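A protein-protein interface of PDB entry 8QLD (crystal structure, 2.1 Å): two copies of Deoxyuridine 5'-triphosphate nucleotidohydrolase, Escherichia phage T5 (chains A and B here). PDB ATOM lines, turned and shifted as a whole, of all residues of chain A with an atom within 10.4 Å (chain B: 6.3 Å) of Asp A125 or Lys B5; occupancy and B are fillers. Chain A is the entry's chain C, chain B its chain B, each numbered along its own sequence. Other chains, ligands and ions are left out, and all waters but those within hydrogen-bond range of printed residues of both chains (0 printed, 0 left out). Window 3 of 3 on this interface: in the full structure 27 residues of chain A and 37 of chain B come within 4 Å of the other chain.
No position is printed for both chains.
Of the 17 pairs that touch across the chains among the printed residues, none has its exchanged pair printed and touching as well.
Asp A125 touches just one residue of chain B: Lys B5 (3.5 Å).
Ile B4 touches four residues of chain A.
Of chain A, only Ile A123 (3.9 Å) comes within 4 Å of Leu B6.
Ala B48 touches just one residue of chain A: Leu A127.
Printed residues of chain B within 4 Å of Thr A130: Arg B84.
Of the printed residues of chain B, Val A124 touches Ile B4 (2.8 Å) and Lys B5 (3.5 Å).
Of the printed residues of chain B, Leu A127 touches Lys B3, Lys B5, Ala B48, Val B49, Glu B50 and Arg B84.
Of the printed residues of chain A, Val B49 touches Leu A127 (3.6 Å).
Of the printed residues of chain B, Ile A123 touches Ile B4 and Leu B6.
The nearest residue of chain A that does not touch Lys B5 is Glu A126 (4.7 Å).
Hydrophobic or aromatic side chains of chain A within 4 Å of the printed part of chain B: Phe A121, Ile A123, Val A124 and Leu A127.
Among the printed residues, 17 pairs touch across the chains.
Among the printed residues, no Asp or Glu carboxylate lies within 4 Å of a Lys or Arg side-chain nitrogen of the other chain.
The backbone carbonyl oxygen (O) of Lys A122 sits at hydrogen-bond distance from the backbone NH (N) of Ile B4 (2.9 Å).
O of Ile B4 lies within hydrogen-bond range of N of Val A124.
The backbone NH (N) of Glu A128 lies within hydrogen-bond range of the side-chain carboxylate (OE1) of Glu B50, 3.1 Å away.
NE of Arg B84 is in hydrogen-bond range of O of Glu A128 (3.0 Å).
O of Lys B3 lies within hydrogen-bond range of N of Glu B50 (2.8 Å).
The backbone NH (N) of Lys B5 sits at hydrogen-bond distance from the backbone carbonyl oxygen (O) of Ala B48 (2.9 Å).
Ile B4 touches Phe A121.
Lys A122 touches Lys B3.
CD1 of Leu B6 touches CG2 of Ile A123, at 3.9 Å.
Lys B5 touches Val A124 (CA to O, 3.5 Å).
Asp A125 touches Lys B5.
Lys B5 touches Leu A127 (CE to CG, 3.9 Å).
CD1 of Leu A127 touches CB of Ala B48, at 3.7 Å.
CD2 of Leu A127 touches CB of Glu B50, at 3.7 Å.
Arg B84 touches Leu A127.
Thr A130 touches Arg B84 (CG2 to NH2, 3.5 Å).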
ATOM      1  N   PHE A 121      -8.843   0.072 -14.288  1.00  0.00           N
ATOM      2  CA  PHE A 121      -7.591  -0.619 -14.566  1.00  0.00           C
ATOM      3  C   PHE A 121      -6.738   0.302 -15.434  1.00  0.00           C
ATOM      4  O   PHE A 121      -7.283   1.233 -16.005  1.00  0.00           O
ATOM      5  CB  PHE A 121      -7.856  -1.959 -15.270  1.00  0.00           C
ATOM      6  CG  PHE A 121      -8.323  -1.797 -16.688  1.00  0.00           C
ATOM      7  CD1 PHE A 121      -9.656  -1.591 -16.978  1.00  0.00           C
ATOM      8  CD2 PHE A 121      -7.408  -1.727 -17.722  1.00  0.00           C
ATOM      9  CE1 PHE A 121     -10.070  -1.347 -18.281  1.00  0.00           C
ATOM     10  CE2 PHE A 121      -7.816  -1.461 -19.023  1.00  0.00           C
ATOM     11  CZ  PHE A 121      -9.150  -1.282 -19.303  1.00  0.00           C
ATOM     12  N   LYS A 122      -5.431   0.028 -15.544  1.00  0.00           N
ATOM     13  CA  LYS A 122      -4.597   0.659 -16.562  1.00  0.00           C
ATOM     14  C   LYS A 122      -3.613  -0.374 -17.127  1.00  0.00           C
ATOM     15  O   LYS A 122      -3.031  -1.140 -16.370  1.00  0.00           O
ATOM     16  CB  LYS A 122      -3.888   1.892 -15.983  1.00  0.00           C
ATOM     17  CG  LYS A 122      -3.061   2.703 -16.979  1.00  0.00           C
ATOM     18  CD  LYS A 122      -2.005   3.630 -16.371  1.00  0.00           C
ATOM     19  CE  LYS A 122      -2.248   5.122 -16.524  1.00  0.00           C
ATOM     20  NZ  LYS A 122      -3.431   5.589 -15.763  1.00  0.00           N
ATOM     21  N   ILE A 123      -3.413  -0.382 -18.457  1.00  0.00           N
ATOM     22  CA  ILE A 123      -2.412  -1.228 -19.094  1.00  0.00           C
ATOM     23  C   ILE A 123      -1.029  -0.624 -18.868  1.00  0.00           C
ATOM     24  O   ILE A 123      -0.858   0.581 -19.015  1.00  0.00           O
ATOM     25  CB  ILE A 123      -2.667  -1.392 -20.605  1.00  0.00           C
ATOM     26  CG1 ILE A 123      -4.143  -1.602 -20.956  1.00  0.00           C
ATOM     27  CG2 ILE A 123      -1.783  -2.475 -21.188  1.00  0.00           C
ATOM     28  CD1 ILE A 123      -4.786  -0.377 -21.612  1.00  0.00           C
ATOM     29  N   VAL A 124      -0.032  -1.462 -18.541  1.00  0.00           N
ATOM     30  CA  VAL A 124       1.334  -0.982 -18.341  1.00  0.00           C
ATOM     31  C   VAL A 124       2.299  -1.964 -18.998  1.00  0.00           C
ATOM     32  O   VAL A 124       1.908  -3.090 -19.295  1.00  0.00           O
ATOM     33  CB  VAL A 124       1.695  -0.808 -16.849  1.00  0.00           C
ATOM     34  CG1 VAL A 124       0.693   0.073 -16.125  1.00  0.00           C
ATOM     35  CG2 VAL A 124       1.853  -2.146 -16.140  1.00  0.00           C
ATOM     36  N   ASP A 125       3.559  -1.535 -19.136  1.00  0.00           N
ATOM     37  CA  ASP A 125       4.622  -2.345 -19.710  1.00  0.00           C
ATOM     38  C   ASP A 125       5.250  -3.224 -18.635  1.00  0.00           C
ATOM     39  O   ASP A 125       5.688  -4.341 -18.915  1.00  0.00           O
ATOM     40  CB  ASP A 125       5.711  -1.476 -20.346  1.00  0.00           C
ATOM     41  CG  ASP A 125       5.143  -0.499 -21.357  1.00  0.00           C
ATOM     42  OD1 ASP A 125       4.195  -0.897 -22.071  1.00  0.00           O
ATOM     43  OD2 ASP A 125       5.636   0.640 -21.423  1.00  0.00           O
ATOM     44  N   GLU A 126       5.320  -2.689 -17.413  1.00  0.00           N
ATOM     45  CA  GLU A 126       6.045  -3.351 -16.347  1.00  0.00           C
ATOM     46  C   GLU A 126       5.207  -3.327 -15.071  1.00  0.00           C
ATOM     47  O   GLU A 126       4.649  -2.294 -14.719  1.00  0.00           O
ATOM     48  CB  GLU A 126       7.401  -2.667 -16.165  1.00  0.00           C
ATOM     49  CG  GLU A 126       8.526  -3.664 -15.978  1.00  0.00           C
ATOM     50  CD  GLU A 126       8.903  -4.426 -17.238  1.00  0.00           C
ATOM     51  OE1 GLU A 126       9.434  -3.793 -18.160  1.00  0.00           O
ATOM     52  OE2 GLU A 126       8.680  -5.650 -17.292  1.00  0.00           O
ATOM     53  N   LEU A 127       5.116  -4.477 -14.387  1.00  0.00           N
ATOM     54  CA  LEU A 127       4.469  -4.530 -13.083  1.00  0.00           C
ATOM     55  C   LEU A 127       5.482  -4.172 -12.005  1.00  0.00           C
ATOM     56  O   LEU A 127       6.664  -4.473 -12.158  1.00  0.00           O
ATOM     57  CB  LEU A 127       3.909  -5.930 -12.820  1.00  0.00           C
ATOM     58  CG  LEU A 127       2.621  -6.284 -13.553  1.00  0.00           C
ATOM     59  CD1 LEU A 127       2.057  -7.581 -13.005  1.00  0.00           C
ATOM     60  CD2 LEU A 127       1.604  -5.155 -13.453  1.00  0.00           C
ATOM     61  N   GLU A 128       4.997  -3.537 -10.927  1.00  0.00           N
ATOM     62  CA  GLU A 128       5.824  -3.249  -9.763  1.00  0.00           C
ATOM     63  C   GLU A 128       6.328  -4.566  -9.180  1.00  0.00           C
ATOM     64  O   GLU A 128       5.599  -5.549  -9.132  1.00  0.00           O
ATOM     65  CB  GLU A 128       5.059  -2.431  -8.719  1.00  0.00           C
ATOM     66  CG  GLU A 128       4.755  -1.005  -9.163  1.00  0.00           C
ATOM     67  CD  GLU A 128       5.958  -0.076  -9.261  1.00  0.00           C
ATOM     68  OE1 GLU A 128       6.233   0.424 -10.369  1.00  0.00           O
ATOM     69  OE2 GLU A 128       6.612   0.163  -8.223  1.00  0.00           O
ATOM     70  N   GLU A 129       7.596  -4.555  -8.760  1.00  0.00           N
ATOM     71  CA  GLU A 129       8.325  -5.727  -8.306  1.00  0.00           C
ATOM     72  C   GLU A 129       7.839  -6.126  -6.913  1.00  0.00           C
ATOM     73  O   GLU A 129       7.539  -5.274  -6.087  1.00  0.00           O
ATOM     74  CB  GLU A 129       9.814  -5.370  -8.276  1.00  0.00           C
ATOM     75  CG  GLU A 129      10.751  -6.553  -8.423  1.00  0.00           C
ATOM     76  CD  GLU A 129      12.203  -6.246  -8.096  1.00  0.00           C
ATOM     77  OE1 GLU A 129      13.079  -6.959  -8.611  1.00  0.00           O
ATOM     78  OE2 GLU A 129      12.457  -5.315  -7.304  1.00  0.00           O
ATOM     79  N   THR A 130       7.721  -7.431  -6.660  1.00  0.00           N
ATOM     80  CA  THR A 130       7.527  -7.936  -5.308  1.00  0.00           C
ATOM     81  C   THR A 130       8.416  -9.157  -5.044  1.00  0.00           C
ATOM     82  O   THR A 130       8.432  -9.657  -3.920  1.00  0.00           O
ATOM     83  CB  THR A 130       6.051  -8.269  -5.017  1.00  0.00           C
ATOM     84  OG1 THR A 130       5.661  -9.445  -5.735  1.00  0.00           O
ATOM     85  CG2 THR A 130       5.105  -7.135  -5.352  1.00  0.00           C
ATOM     86  N   LYS B   3      -3.461  -2.634 -12.178  1.00  0.00           N
ATOM     87  CA  LYS B   3      -2.481  -2.471 -13.231  1.00  0.00           C
ATOM     88  C   LYS B   3      -2.406  -3.799 -13.965  1.00  0.00           C
ATOM     89  O   LYS B   3      -2.324  -4.846 -13.323  1.00  0.00           O
ATOM     90  CB  LYS B   3      -1.109  -2.066 -12.682  1.00  0.00           C
ATOM     91  CG  LYS B   3      -0.998  -0.686 -12.044  1.00  0.00           C
ATOM     92  CD  LYS B   3       0.451  -0.194 -12.031  1.00  0.00           C
ATOM     93  CE  LYS B   3       0.857   0.613 -10.811  1.00  0.00           C
ATOM     94  NZ  LYS B   3      -0.017   1.788 -10.596  1.00  0.00           N
ATOM     95  N   ILE B   4      -2.442  -3.735 -15.298  1.00  0.00           N
ATOM     96  CA  ILE B   4      -2.444  -4.928 -16.133  1.00  0.00           C
ATOM     97  C   ILE B   4      -1.286  -4.861 -17.130  1.00  0.00           C
ATOM     98  O   ILE B   4      -1.167  -3.891 -17.878  1.00  0.00           O
ATOM     99  CB  ILE B   4      -3.793  -5.060 -16.866  1.00  0.00           C
ATOM    100  CG1 ILE B   4      -4.976  -5.160 -15.900  1.00  0.00           C
ATOM    101  CG2 ILE B   4      -3.752  -6.217 -17.843  1.00  0.00           C
ATOM    102  CD1 ILE B   4      -6.327  -5.145 -16.590  1.00  0.00           C
ATOM    103  N   LYS B   5      -0.470  -5.923 -17.171  1.00  0.00           N
ATOM    104  CA  LYS B   5       0.517  -6.104 -18.220  1.00  0.00           C
ATOM    105  C   LYS B   5       0.094  -7.255 -19.119  1.00  0.00           C
ATOM    106  O   LYS B   5      -0.142  -8.368 -18.642  1.00  0.00           O
ATOM    107  CB  LYS B   5       1.896  -6.403 -17.637  1.00  0.00           C
ATOM    108  CG  LYS B   5       2.871  -7.066 -18.607  1.00  0.00           C
ATOM    109  CD  LYS B   5       4.233  -7.346 -18.021  1.00  0.00           C
ATOM    110  CE  LYS B   5       4.117  -8.063 -16.691  1.00  0.00           C
ATOM    111  NZ  LYS B   5       5.346  -8.819 -16.362  1.00  0.00           N
ATOM    112  N   LEU B   6       0.065  -6.979 -20.426  1.00  0.00           N
ATOM    113  CA  LEU B   6      -0.396  -7.918 -21.434  1.00  0.00           C
ATOM    114  C   LEU B   6       0.808  -8.480 -22.180  1.00  0.00           C
ATOM    115  O   LEU B   6       1.663  -7.740 -22.635  1.00  0.00           O
ATOM    116  CB  LEU B   6      -1.338  -7.190 -22.404  1.00  0.00           C
ATOM    117  CG  LEU B   6      -2.579  -6.530 -21.797  1.00  0.00           C
ATOM    118  CD1 LEU B   6      -3.280  -5.663 -22.836  1.00  0.00           C
ATOM    119  CD2 LEU B   6      -3.544  -7.572 -21.228  1.00  0.00           C
ATOM    120  N   THR B   7       0.862  -9.802 -22.325  1.00  0.00           N
ATOM    121  CA  THR B   7       1.874 -10.431 -23.162  1.00  0.00           C
ATOM    122  C   THR B   7       1.679 -10.025 -24.626  1.00  0.00           C
ATOM    123  O   THR B   7       2.640  -9.863 -25.375  1.00  0.00           O
ATOM    124  CB  THR B   7       1.835 -11.951 -22.994  1.00  0.00           C
ATOM    125  OG1 THR B   7       2.058 -12.252 -21.616  1.00  0.00           O
ATOM    126  CG2 THR B   7       2.861 -12.657 -23.854  1.00  0.00           C
ATOM    127  N   GLY B  46      -1.760 -14.771 -20.577  1.00  0.00           N
ATOM    128  CA  GLY B  46      -0.954 -13.642 -21.010  1.00  0.00           C
ATOM    129  C   GLY B  46      -1.309 -12.338 -20.288  1.00  0.00           C
ATOM    130  O   GLY B  46      -0.922 -11.257 -20.734  1.00  0.00           O
ATOM    131  N   VAL B  47      -2.083 -12.455 -19.204  1.00  0.00           N
ATOM    132  CA  VAL B  47      -2.442 -11.327 -18.366  1.00  0.00           C
ATOM    133  C   VAL B  47      -1.765 -11.478 -17.005  1.00  0.00           C
ATOM    134  O   VAL B  47      -2.121 -12.366 -16.244  1.00  0.00           O
ATOM    135  CB  VAL B  47      -3.965 -11.210 -18.208  1.00  0.00           C
ATOM    136  CG1 VAL B  47      -4.326 -10.101 -17.244  1.00  0.00           C
ATOM    137  CG2 VAL B  47      -4.646 -10.993 -19.544  1.00  0.00           C
ATOM    138  N   ALA B  48      -0.804 -10.590 -16.725  1.00  0.00           N
ATOM    139  CA  ALA B  48      -0.251 -10.369 -15.394  1.00  0.00           C
ATOM    140  C   ALA B  48      -0.902  -9.133 -14.780  1.00  0.00           C
ATOM    141  O   ALA B  48      -1.125  -8.130 -15.455  1.00  0.00           O
ATOM    142  CB  ALA B  48       1.243 -10.188 -15.488  1.00  0.00           C
ATOM    143  N   VAL B  49      -1.224  -9.203 -13.491  1.00  0.00           N
ATOM    144  CA  VAL B  49      -1.990  -8.150 -12.848  1.00  0.00           C
ATOM    145  C   VAL B  49      -1.296  -7.758 -11.559  1.00  0.00           C
ATOM    146  O   VAL B  49      -0.655  -8.596 -10.913  1.00  0.00           O
ATOM    147  CB  VAL B  49      -3.447  -8.559 -12.548  1.00  0.00           C
ATOM    148  CG1 VAL B  49      -4.265  -8.774 -13.815  1.00  0.00           C
ATOM    149  CG2 VAL B  49      -3.521  -9.774 -11.636  1.00  0.00           C
ATOM    150  N   GLU B  50      -1.456  -6.464 -11.235  1.00  0.00           N
ATOM    151  CA  GLU B  50      -1.124  -5.908  -9.947  1.00  0.00           C
ATOM    152  C   GLU B  50      -2.446  -5.483  -9.307  1.00  0.00           C
ATOM    153  O   GLU B  50      -3.047  -4.460  -9.648  1.00  0.00           O
ATOM    154  CB  GLU B  50      -0.080  -4.811 -10.159  1.00  0.00           C
ATOM    155  CG  GLU B  50       0.085  -3.873  -8.988  1.00  0.00           C
ATOM    156  CD  GLU B  50       1.192  -2.840  -9.161  1.00  0.00           C
ATOM    157  OE1 GLU B  50       2.125  -3.043 -10.001  1.00  0.00           O
ATOM    158  OE2 GLU B  50       1.115  -1.823  -8.467  1.00  0.00           O
ATOM    159  N   ARG B  84       2.787 -11.707  -9.420  1.00  0.00           N
ATOM    160  CA  ARG B  84       3.237 -10.898 -10.550  1.00  0.00           C
ATOM    161  C   ARG B  84       3.428 -11.705 -11.839  1.00  0.00           C
ATOM    162  O   ARG B  84       3.787 -11.131 -12.863  1.00  0.00           O
ATOM    163  CB  ARG B  84       4.516 -10.157 -10.177  1.00  0.00           C
ATOM    164  CG  ARG B  84       4.300  -9.082  -9.127  1.00  0.00           C
ATOM    165  CD  ARG B  84       3.350  -7.987  -9.582  1.00  0.00           C
ATOM    166  NE  ARG B  84       3.092  -7.055  -8.492  1.00  0.00           N
ATOM    167  CZ  ARG B  84       2.037  -7.078  -7.680  1.00  0.00           C
ATOM    168  NH1 ARG B  84       1.050  -7.938  -7.867  1.00  0.00           N
ATOM    169  NH2 ARG B  84       1.975  -6.221  -6.671  1.00  0.00           N
ATOM    170  N   THR B  86       1.786 -14.263 -15.000  1.00  0.00           N
ATOM    171  CA  THR B  86       0.538 -14.213 -15.737  1.00  0.00           C
ATOM    172  C   THR B  86      -0.414 -15.189 -15.067  1.00  0.00           C
ATOM    173  O   THR B  86       0.007 -16.215 -14.541  1.00  0.00           O
ATOM    174  CB  THR B  86       0.744 -14.465 -17.239  1.00  0.00           C
ATOM    175  OG1 THR B  86       1.043 -15.845 -17.451  1.00  0.00           O
ATOM    176  CG2 THR B  86       1.812 -13.562 -17.820  1.00  0.00           C
